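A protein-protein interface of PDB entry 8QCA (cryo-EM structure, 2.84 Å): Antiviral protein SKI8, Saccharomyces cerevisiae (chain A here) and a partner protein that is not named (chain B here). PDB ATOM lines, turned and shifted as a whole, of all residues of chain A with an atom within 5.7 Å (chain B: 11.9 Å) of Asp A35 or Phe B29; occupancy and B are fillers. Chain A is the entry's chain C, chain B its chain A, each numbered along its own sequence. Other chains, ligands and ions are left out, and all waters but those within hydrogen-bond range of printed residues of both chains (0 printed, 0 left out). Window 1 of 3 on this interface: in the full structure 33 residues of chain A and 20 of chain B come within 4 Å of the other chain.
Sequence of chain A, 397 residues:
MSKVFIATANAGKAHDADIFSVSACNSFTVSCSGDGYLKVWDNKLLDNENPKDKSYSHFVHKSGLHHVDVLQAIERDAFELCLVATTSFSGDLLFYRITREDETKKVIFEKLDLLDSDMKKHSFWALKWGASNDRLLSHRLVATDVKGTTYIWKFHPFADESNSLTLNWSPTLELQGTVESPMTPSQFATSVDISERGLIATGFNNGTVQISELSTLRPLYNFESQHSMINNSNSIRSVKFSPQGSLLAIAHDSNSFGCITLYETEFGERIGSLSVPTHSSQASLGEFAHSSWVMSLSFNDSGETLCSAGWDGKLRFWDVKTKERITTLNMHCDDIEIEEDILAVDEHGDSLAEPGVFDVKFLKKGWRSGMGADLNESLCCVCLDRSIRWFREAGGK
Phe B29 touches Asp A16.
CG of Phe B29 touches CB of Asp A35, 3.7 Å away.
CE2 of Phe A59 touches OD1 of Asn B22, 3.2 Å away.
Ile B20 touches His A61 (O to CE1, 3.6 Å).
OD2 of Asp A35 lies within hydrogen-bond range of N of Asp A16, at 3.3 Å.
The side-chain hydroxyl of Ser A33 sits close to the side-chain carboxylate of Asp A35 (3.5 Å).
The backbone NH of Tyr A37 is in hydrogen-bond range of the side-chain carboxylate of Asp A35 (3.4 Å).
Phe B29 touches just these residues of chain A: Asp A16 and Asp A35.
No residue of chain B comes within 4 Å of His A15.
Asp A16 touches just one residue of chain B: Phe B29 (3.8 Å).
No residue of chain B comes within 4 Å of Ser A33.
No residue of chain B comes within 4 Å of Gly A34.
No residue of chain B comes within 4 Å of Tyr A37.
Of the printed residues of chain A, Asn B22 touches Phe A59 (3.2 Å) and Lys A62 (3.5 Å).
Of the printed residues of chain B, His A61 touches Ile B20 (3.6 Å).
Of the printed residues of chain A, Ile B20 touches His A61.
Of the printed residues of chain B, Phe A59 touches Asn B22.
Ala B24 touches none of the printed residues of chain A.
Glu B30 touches none of the printed residues of chain A.
The nearest residue of chain A that does not touch Phe B29 is Ala A17 (4.5 Å).
OD1 of Asn B22 lies within hydrogen-bond range of N of Lys A62 (3.5 Å).
Along chain B the printed residues that touch a printed residue of chain A span positions 20 to 29.
Among the printed residues, 5 pairs touch across the chains.
Among the printed residues, no Asp or Glu carboxylate lies within 4 Å of a Lys or Arg side-chain nitrogen of the other chain.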
ATOM      1  N   HIS A  15      16.897  14.156  19.263  1.00  0.00           N
ATOM      2  CA  HIS A  15      17.253  15.464  18.737  1.00  0.00           C
ATOM      3  C   HIS A  15      18.242  15.308  17.588  1.00  0.00           C
ATOM      4  O   HIS A  15      18.820  14.240  17.374  1.00  0.00           O
ATOM      5  CB  HIS A  15      17.846  16.349  19.837  1.00  0.00           C
ATOM      6  CG  HIS A  15      16.822  16.992  20.722  1.00  0.00           C
ATOM      7  ND1 HIS A  15      16.172  18.159  20.383  1.00  0.00           N
ATOM      8  CD2 HIS A  15      16.348  16.639  21.939  1.00  0.00           C
ATOM      9  CE1 HIS A  15      15.337  18.493  21.351  1.00  0.00           C
ATOM     10  NE2 HIS A  15      15.424  17.586  22.307  1.00  0.00           N
ATOM     11  N   ASP A  16      18.431  16.394  16.839  1.00  0.00           N
ATOM     12  CA  ASP A  16      19.365  16.398  15.720  1.00  0.00           C
ATOM     13  C   ASP A  16      20.780  16.790  16.118  1.00  0.00           C
ATOM     14  O   ASP A  16      21.709  16.582  15.331  1.00  0.00           O
ATOM     15  CB  ASP A  16      18.878  17.346  14.620  1.00  0.00           C
ATOM     16  CG  ASP A  16      17.887  16.690  13.682  1.00  0.00           C
ATOM     17  OD1 ASP A  16      18.018  15.474  13.435  1.00  0.00           O
ATOM     18  OD2 ASP A  16      16.976  17.389  13.192  1.00  0.00           O
ATOM     19  N   ALA A  17      20.968  17.348  17.310  1.00  0.00           N
ATOM     20  CA  ALA A  17      22.283  17.759  17.780  1.00  0.00           C
ATOM     21  C   ALA A  17      22.401  17.374  19.250  1.00  0.00           C
ATOM     22  O   ALA A  17      21.516  16.722  19.812  1.00  0.00           O
ATOM     23  CB  ALA A  17      22.503  19.259  17.546  1.00  0.00           C
ATOM     24  N   ASP A  18      23.505  17.782  19.873  1.00  0.00           N
ATOM     25  CA  ASP A  18      23.762  17.431  21.263  1.00  0.00           C
ATOM     26  C   ASP A  18      22.661  17.965  22.171  1.00  0.00           C
ATOM     27  O   ASP A  18      22.265  19.129  22.069  1.00  0.00           O
ATOM     28  CB  ASP A  18      25.114  17.989  21.704  1.00  0.00           C
ATOM     29  CG  ASP A  18      26.271  17.365  20.961  1.00  0.00           C
ATOM     30  OD1 ASP A  18      26.125  16.222  20.483  1.00  0.00           O
ATOM     31  OD2 ASP A  18      27.327  18.023  20.852  1.00  0.00           O
ATOM     32  N   SER A  33      18.396  21.299  22.840  1.00  0.00           N
ATOM     33  CA  SER A  33      19.487  20.777  22.034  1.00  0.00           C
ATOM     34  C   SER A  33      20.156  21.913  21.275  1.00  0.00           C
ATOM     35  O   SER A  33      19.684  23.052  21.268  1.00  0.00           O
ATOM     36  CB  SER A  33      18.992  19.701  21.059  1.00  0.00           C
ATOM     37  OG  SER A  33      20.072  19.085  20.382  1.00  0.00           O
ATOM     38  N   GLY A  34      21.274  21.588  20.631  1.00  0.00           N
ATOM     39  CA  GLY A  34      22.002  22.562  19.843  1.00  0.00           C
ATOM     40  C   GLY A  34      21.402  22.873  18.490  1.00  0.00           C
ATOM     41  O   GLY A  34      21.879  23.790  17.816  1.00  0.00           O
ATOM     42  N   ASP A  35      20.373  22.137  18.076  1.00  0.00           N
ATOM     43  CA  ASP A  35      19.687  22.423  16.823  1.00  0.00           C
ATOM     44  C   ASP A  35      18.611  23.491  16.971  1.00  0.00           C
ATOM     45  O   ASP A  35      17.966  23.840  15.977  1.00  0.00           O
ATOM     46  CB  ASP A  35      19.078  21.141  16.245  1.00  0.00           C
ATOM     47  CG  ASP A  35      18.081  20.488  17.181  1.00  0.00           C
ATOM     48  OD1 ASP A  35      17.939  20.950  18.330  1.00  0.00           O
ATOM     49  OD2 ASP A  35      17.436  19.505  16.763  1.00  0.00           O
ATOM     50  N   GLY A  36      18.402  24.010  18.178  1.00  0.00           N
ATOM     51  CA  GLY A  36      17.480  25.105  18.388  1.00  0.00           C
ATOM     52  C   GLY A  36      16.053  24.717  18.686  1.00  0.00           C
ATOM     53  O   GLY A  36      15.178  25.589  18.674  1.00  0.00           O
ATOM     54  N   TYR A  37      15.783  23.445  18.952  1.00  0.00           N
ATOM     55  CA  TYR A  37      14.438  22.987  19.255  1.00  0.00           C
ATOM     56  C   TYR A  37      14.265  22.758  20.748  1.00  0.00           C
ATOM     57  O   TYR A  37      15.231  22.639  21.506  1.00  0.00           O
ATOM     58  CB  TYR A  37      14.098  21.704  18.490  1.00  0.00           C
ATOM     59  CG  TYR A  37      13.514  21.953  17.122  1.00  0.00           C
ATOM     60  CD1 TYR A  37      12.146  21.880  16.912  1.00  0.00           C
ATOM     61  CD2 TYR A  37      14.325  22.268  16.044  1.00  0.00           C
ATOM     62  CE1 TYR A  37      11.602  22.109  15.669  1.00  0.00           C
ATOM     63  CE2 TYR A  37      13.791  22.499  14.795  1.00  0.00           C
ATOM     64  CZ  TYR A  37      12.428  22.418  14.614  1.00  0.00           C
ATOM     65  OH  TYR A  37      11.887  22.646  13.370  1.00  0.00           O
ATOM     66  N   PHE A  59      10.539  25.457  17.750  1.00  0.00           N
ATOM     67  CA  PHE A  59      11.810  26.074  17.390  1.00  0.00           C
ATOM     68  C   PHE A  59      11.944  27.424  18.082  1.00  0.00           C
ATOM     69  O   PHE A  59      11.019  28.241  18.043  1.00  0.00           O
ATOM     70  CB  PHE A  59      11.914  26.241  15.874  1.00  0.00           C
ATOM     71  CG  PHE A  59      13.145  26.976  15.425  1.00  0.00           C
ATOM     72  CD1 PHE A  59      14.366  26.327  15.352  1.00  0.00           C
ATOM     73  CD2 PHE A  59      13.081  28.310  15.066  1.00  0.00           C
ATOM     74  CE1 PHE A  59      15.498  26.997  14.936  1.00  0.00           C
ATOM     75  CE2 PHE A  59      14.210  28.984  14.651  1.00  0.00           C
ATOM     76  CZ  PHE A  59      15.419  28.327  14.586  1.00  0.00           C
ATOM     77  N   HIS A  61      15.620  29.269  18.741  1.00  0.00           N
ATOM     78  CA  HIS A  61      16.723  30.091  18.264  1.00  0.00           C
ATOM     79  C   HIS A  61      17.606  29.291  17.320  1.00  0.00           C
ATOM     80  O   HIS A  61      17.855  28.105  17.547  1.00  0.00           O
ATOM     81  CB  HIS A  61      17.562  30.629  19.429  1.00  0.00           C
ATOM     82  CG  HIS A  61      18.255  31.920  19.127  1.00  0.00           C
ATOM     83  ND1 HIS A  61      19.319  32.008  18.255  1.00  0.00           N
ATOM     84  CD2 HIS A  61      18.033  33.178  19.575  1.00  0.00           C
ATOM     85  CE1 HIS A  61      19.725  33.262  18.183  1.00  0.00           C
ATOM     86  NE2 HIS A  61      18.961  33.993  18.974  1.00  0.00           N
ATOM     87  N   LYS A  62      18.086  29.956  16.269  1.00  0.00           N
ATOM     88  CA  LYS A  62      18.929  29.299  15.277  1.00  0.00           C
ATOM     89  C   LYS A  62      20.303  28.934  15.821  1.00  0.00           C
ATOM     90  O   LYS A  62      20.955  28.043  15.269  1.00  0.00           O
ATOM     91  CB  LYS A  62      19.084  30.193  14.046  1.00  0.00           C
ATOM     92  N   GLY A  64      20.954  27.615  18.758  1.00  0.00           N
ATOM     93  CA  GLY A  64      20.889  26.489  19.663  1.00  0.00           C
ATOM     94  C   GLY A  64      20.698  26.910  21.111  1.00  0.00           C
ATOM     95  O   GLY A  64      20.881  28.065  21.487  1.00  0.00           O
ATOM     96  N   LEU A  65      20.323  25.936  21.934  1.00  0.00           N
ATOM     97  CA  LEU A  65      20.063  26.150  23.349  1.00  0.00           C
ATOM     98  C   LEU A  65      20.909  25.189  24.173  1.00  0.00           C
ATOM     99  O   LEU A  65      21.184  24.063  23.748  1.00  0.00           O
ATOM    100  CB  LEU A  65      18.580  25.946  23.670  1.00  0.00           C
ATOM    101  CG  LEU A  65      17.574  26.690  22.788  1.00  0.00           C
ATOM    102  CD1 LEU A  65      16.166  26.201  23.061  1.00  0.00           C
ATOM    103  CD2 LEU A  65      17.670  28.190  22.998  1.00  0.00           C
ATOM    104  N   ILE B  20      23.212  37.767  15.882  1.00  0.00           N
ATOM    105  CA  ILE B  20      22.673  36.628  15.148  1.00  0.00           C
ATOM    106  C   ILE B  20      21.160  36.620  15.311  1.00  0.00           C
ATOM    107  O   ILE B  20      20.641  36.273  16.379  1.00  0.00           O
ATOM    108  CB  ILE B  20      23.297  35.306  15.633  1.00  0.00           C
ATOM    109  CG1 ILE B  20      24.792  35.274  15.308  1.00  0.00           C
ATOM    110  CG2 ILE B  20      22.588  34.116  15.007  1.00  0.00           C
ATOM    111  CD1 ILE B  20      25.550  34.175  16.017  1.00  0.00           C
ATOM    112  N   ASN B  22      17.250  35.517  14.492  1.00  0.00           N
ATOM    113  CA  ASN B  22      16.443  34.389  14.050  1.00  0.00           C
ATOM    114  C   ASN B  22      15.659  34.755  12.795  1.00  0.00           C
ATOM    115  O   ASN B  22      15.130  35.864  12.676  1.00  0.00           O
ATOM    116  CB  ASN B  22      15.490  33.955  15.161  1.00  0.00           C
ATOM    117  CG  ASN B  22      15.120  32.490  15.072  1.00  0.00           C
ATOM    118  OD1 ASN B  22      15.785  31.712  14.391  1.00  0.00           O
ATOM    119  ND2 ASN B  22      14.053  32.107  15.762  1.00  0.00           N
ATOM    120  N   ASN B  23      15.588  33.818  11.859  1.00  0.00           N
ATOM    121  CA  ASN B  23      14.885  34.008  10.598  1.00  0.00           C
ATOM    122  C   ASN B  23      13.734  33.011  10.495  1.00  0.00           C
ATOM    123  O   ASN B  23      13.473  32.229  11.413  1.00  0.00           O
ATOM    124  CB  ASN B  23      15.846  33.864   9.413  1.00  0.00           C
ATOM    125  CG  ASN B  23      16.153  32.417   9.083  1.00  0.00           C
ATOM    126  OD1 ASN B  23      15.454  31.785   8.290  1.00  0.00           O
ATOM    127  ND2 ASN B  23      17.204  31.880   9.693  1.00  0.00           N
ATOM    128  N   ALA B  24      13.045  33.045   9.360  1.00  0.00           N
ATOM    129  CA  ALA B  24      11.924  32.145   9.115  1.00  0.00           C
ATOM    130  C   ALA B  24      12.364  30.940   8.290  1.00  0.00           C
ATOM    131  O   ALA B  24      11.571  30.363   7.545  1.00  0.00           O
ATOM    132  CB  ALA B  24      10.794  32.883   8.417  1.00  0.00           C
ATOM    133  N   LEU B  28      14.513  23.762   8.998  1.00  0.00           N
ATOM    134  CA  LEU B  28      15.148  22.536   9.467  1.00  0.00           C
ATOM    135  C   LEU B  28      16.603  22.785   9.848  1.00  0.00           C
ATOM    136  O   LEU B  28      17.229  23.727   9.363  1.00  0.00           O
ATOM    137  CB  LEU B  28      15.061  21.446   8.397  1.00  0.00           C
ATOM    138  N   PHE B  29      17.136  21.934  10.722  1.00  0.00           N
ATOM    139  CA  PHE B  29      18.518  22.071  11.156  1.00  0.00           C
ATOM    140  C   PHE B  29      19.476  21.757  10.015  1.00  0.00           C
ATOM    141  O   PHE B  29      19.265  20.814   9.245  1.00  0.00           O
ATOM    142  CB  PHE B  29      18.800  21.149  12.341  1.00  0.00           C
ATOM    143  CG  PHE B  29      20.251  21.079  12.723  1.00  0.00           C
ATOM    144  CD1 PHE B  29      20.928  22.212  13.137  1.00  0.00           C
ATOM    145  CD2 PHE B  29      20.938  19.880  12.665  1.00  0.00           C
ATOM    146  CE1 PHE B  29      22.264  22.150  13.487  1.00  0.00           C
ATOM    147  CE2 PHE B  29      22.272  19.813  13.014  1.00  0.00           C
ATOM    148  CZ  PHE B  29      22.935  20.950  13.426  1.00  0.00           C
ATOM    149  N   GLU B  30      20.535  22.555   9.907  1.00  0.00           N
ATOM    150  CA  GLU B  30      21.583  22.350   8.917  1.00  0.00           C
ATOM    151  C   GLU B  30      22.931  22.366   9.616  1.00  0.00           C
ATOM    152  O   GLU B  30      23.228  23.295  10.373  1.00  0.00           O
ATOM    153  CB  GLU B  30      21.536  23.426   7.827  1.00  0.00           C
ATOM    154  N   ASP B  31      23.742  21.342   9.363  1.00  0.00           N
ATOM    155  CA  ASP B  31      25.073  21.247   9.953  1.00  0.00           C
ATOM    156  C   ASP B  31      26.005  22.190   9.205  1.00  0.00           C
ATOM    157  O   ASP B  31      26.435  21.891   8.086  1.00  0.00           O
ATOM    158  CB  ASP B  31      25.577  19.808   9.902  1.00  0.00           C
ATOM    159  CG  ASP B  31      26.656  19.534  10.926  1.00  0.00           C
ATOM    160  OD1 ASP B  31      26.867  20.391  11.807  1.00  0.00           O
ATOM    161  OD2 ASP B  31      27.290  18.462  10.851  1.00  0.00           O
ATOM    162  N   ARG B  32      26.320  23.324   9.817  1.00  0.00           N
ATOM    163  CA  ARG B  32      27.065  24.379   9.152  1.00  0.00           C
ATOM    164  C   ARG B  32      28.564  24.231   9.392  1.00  0.00           C
ATOM    165  O   ARG B  32      29.010  23.549  10.317  1.00  0.00           O
ATOM    166  CB  ARG B  32      26.586  25.748   9.633  1.00  0.00           C
ATOM    167  CG  ARG B  32      25.181  26.092   9.179  1.00  0.00           C
ATOM    168  CD  ARG B  32      24.471  26.967  10.193  1.00  0.00           C
ATOM    169  NE  ARG B  32      23.619  27.959   9.548  1.00  0.00           N
ATOM    170  CZ  ARG B  32      22.485  28.417  10.059  1.00  0.00           C
ATOM    171  NH1 ARG B  32      22.029  27.990  11.225  1.00  0.00           N
ATOM    172  NH2 ARG B  32      21.789  29.327   9.382  1.00  0.00           N
ATOM    173  N   ILE B  33      29.342  24.887   8.534  1.00  0.00           N
ATOM    174  CA  ILE B  33      30.798  24.855   8.584  1.00  0.00           C
ATOM    175  C   ILE B  33      31.299  26.280   8.768  1.00  0.00           C
ATOM    176  O   ILE B  33      30.871  27.192   8.049  1.00  0.00           O
ATOM    177  CB  ILE B  33      31.393  24.216   7.317  1.00  0.00           C
ATOM    178  CG1 ILE B  33      30.990  22.744   7.228  1.00  0.00           C
ATOM    179  CG2 ILE B  33      32.906  24.357   7.299  1.00  0.00           C
ATOM    180  CD1 ILE B  33      31.297  22.108   5.893  1.00  0.00           C
ATOM    181  N   THR B  34      32.198  26.469   9.728  1.00  0.00           N
ATOM    182  CA  THR B  34      32.693  27.799  10.049  1.00  0.00           C
ATOM    183  C   THR B  34      33.555  28.351   8.922  1.00  0.00           C
ATOM    184  O   THR B  34      34.154  27.606   8.142  1.00  0.00           O
ATOM    185  CB  THR B  34      33.502  27.768  11.345  1.00  0.00           C
ATOM    186  OG1 THR B  34      34.011  29.078  11.623  1.00  0.00           O
ATOM    187  CG2 THR B  34      34.663  26.794  11.225  1.00  0.00           C
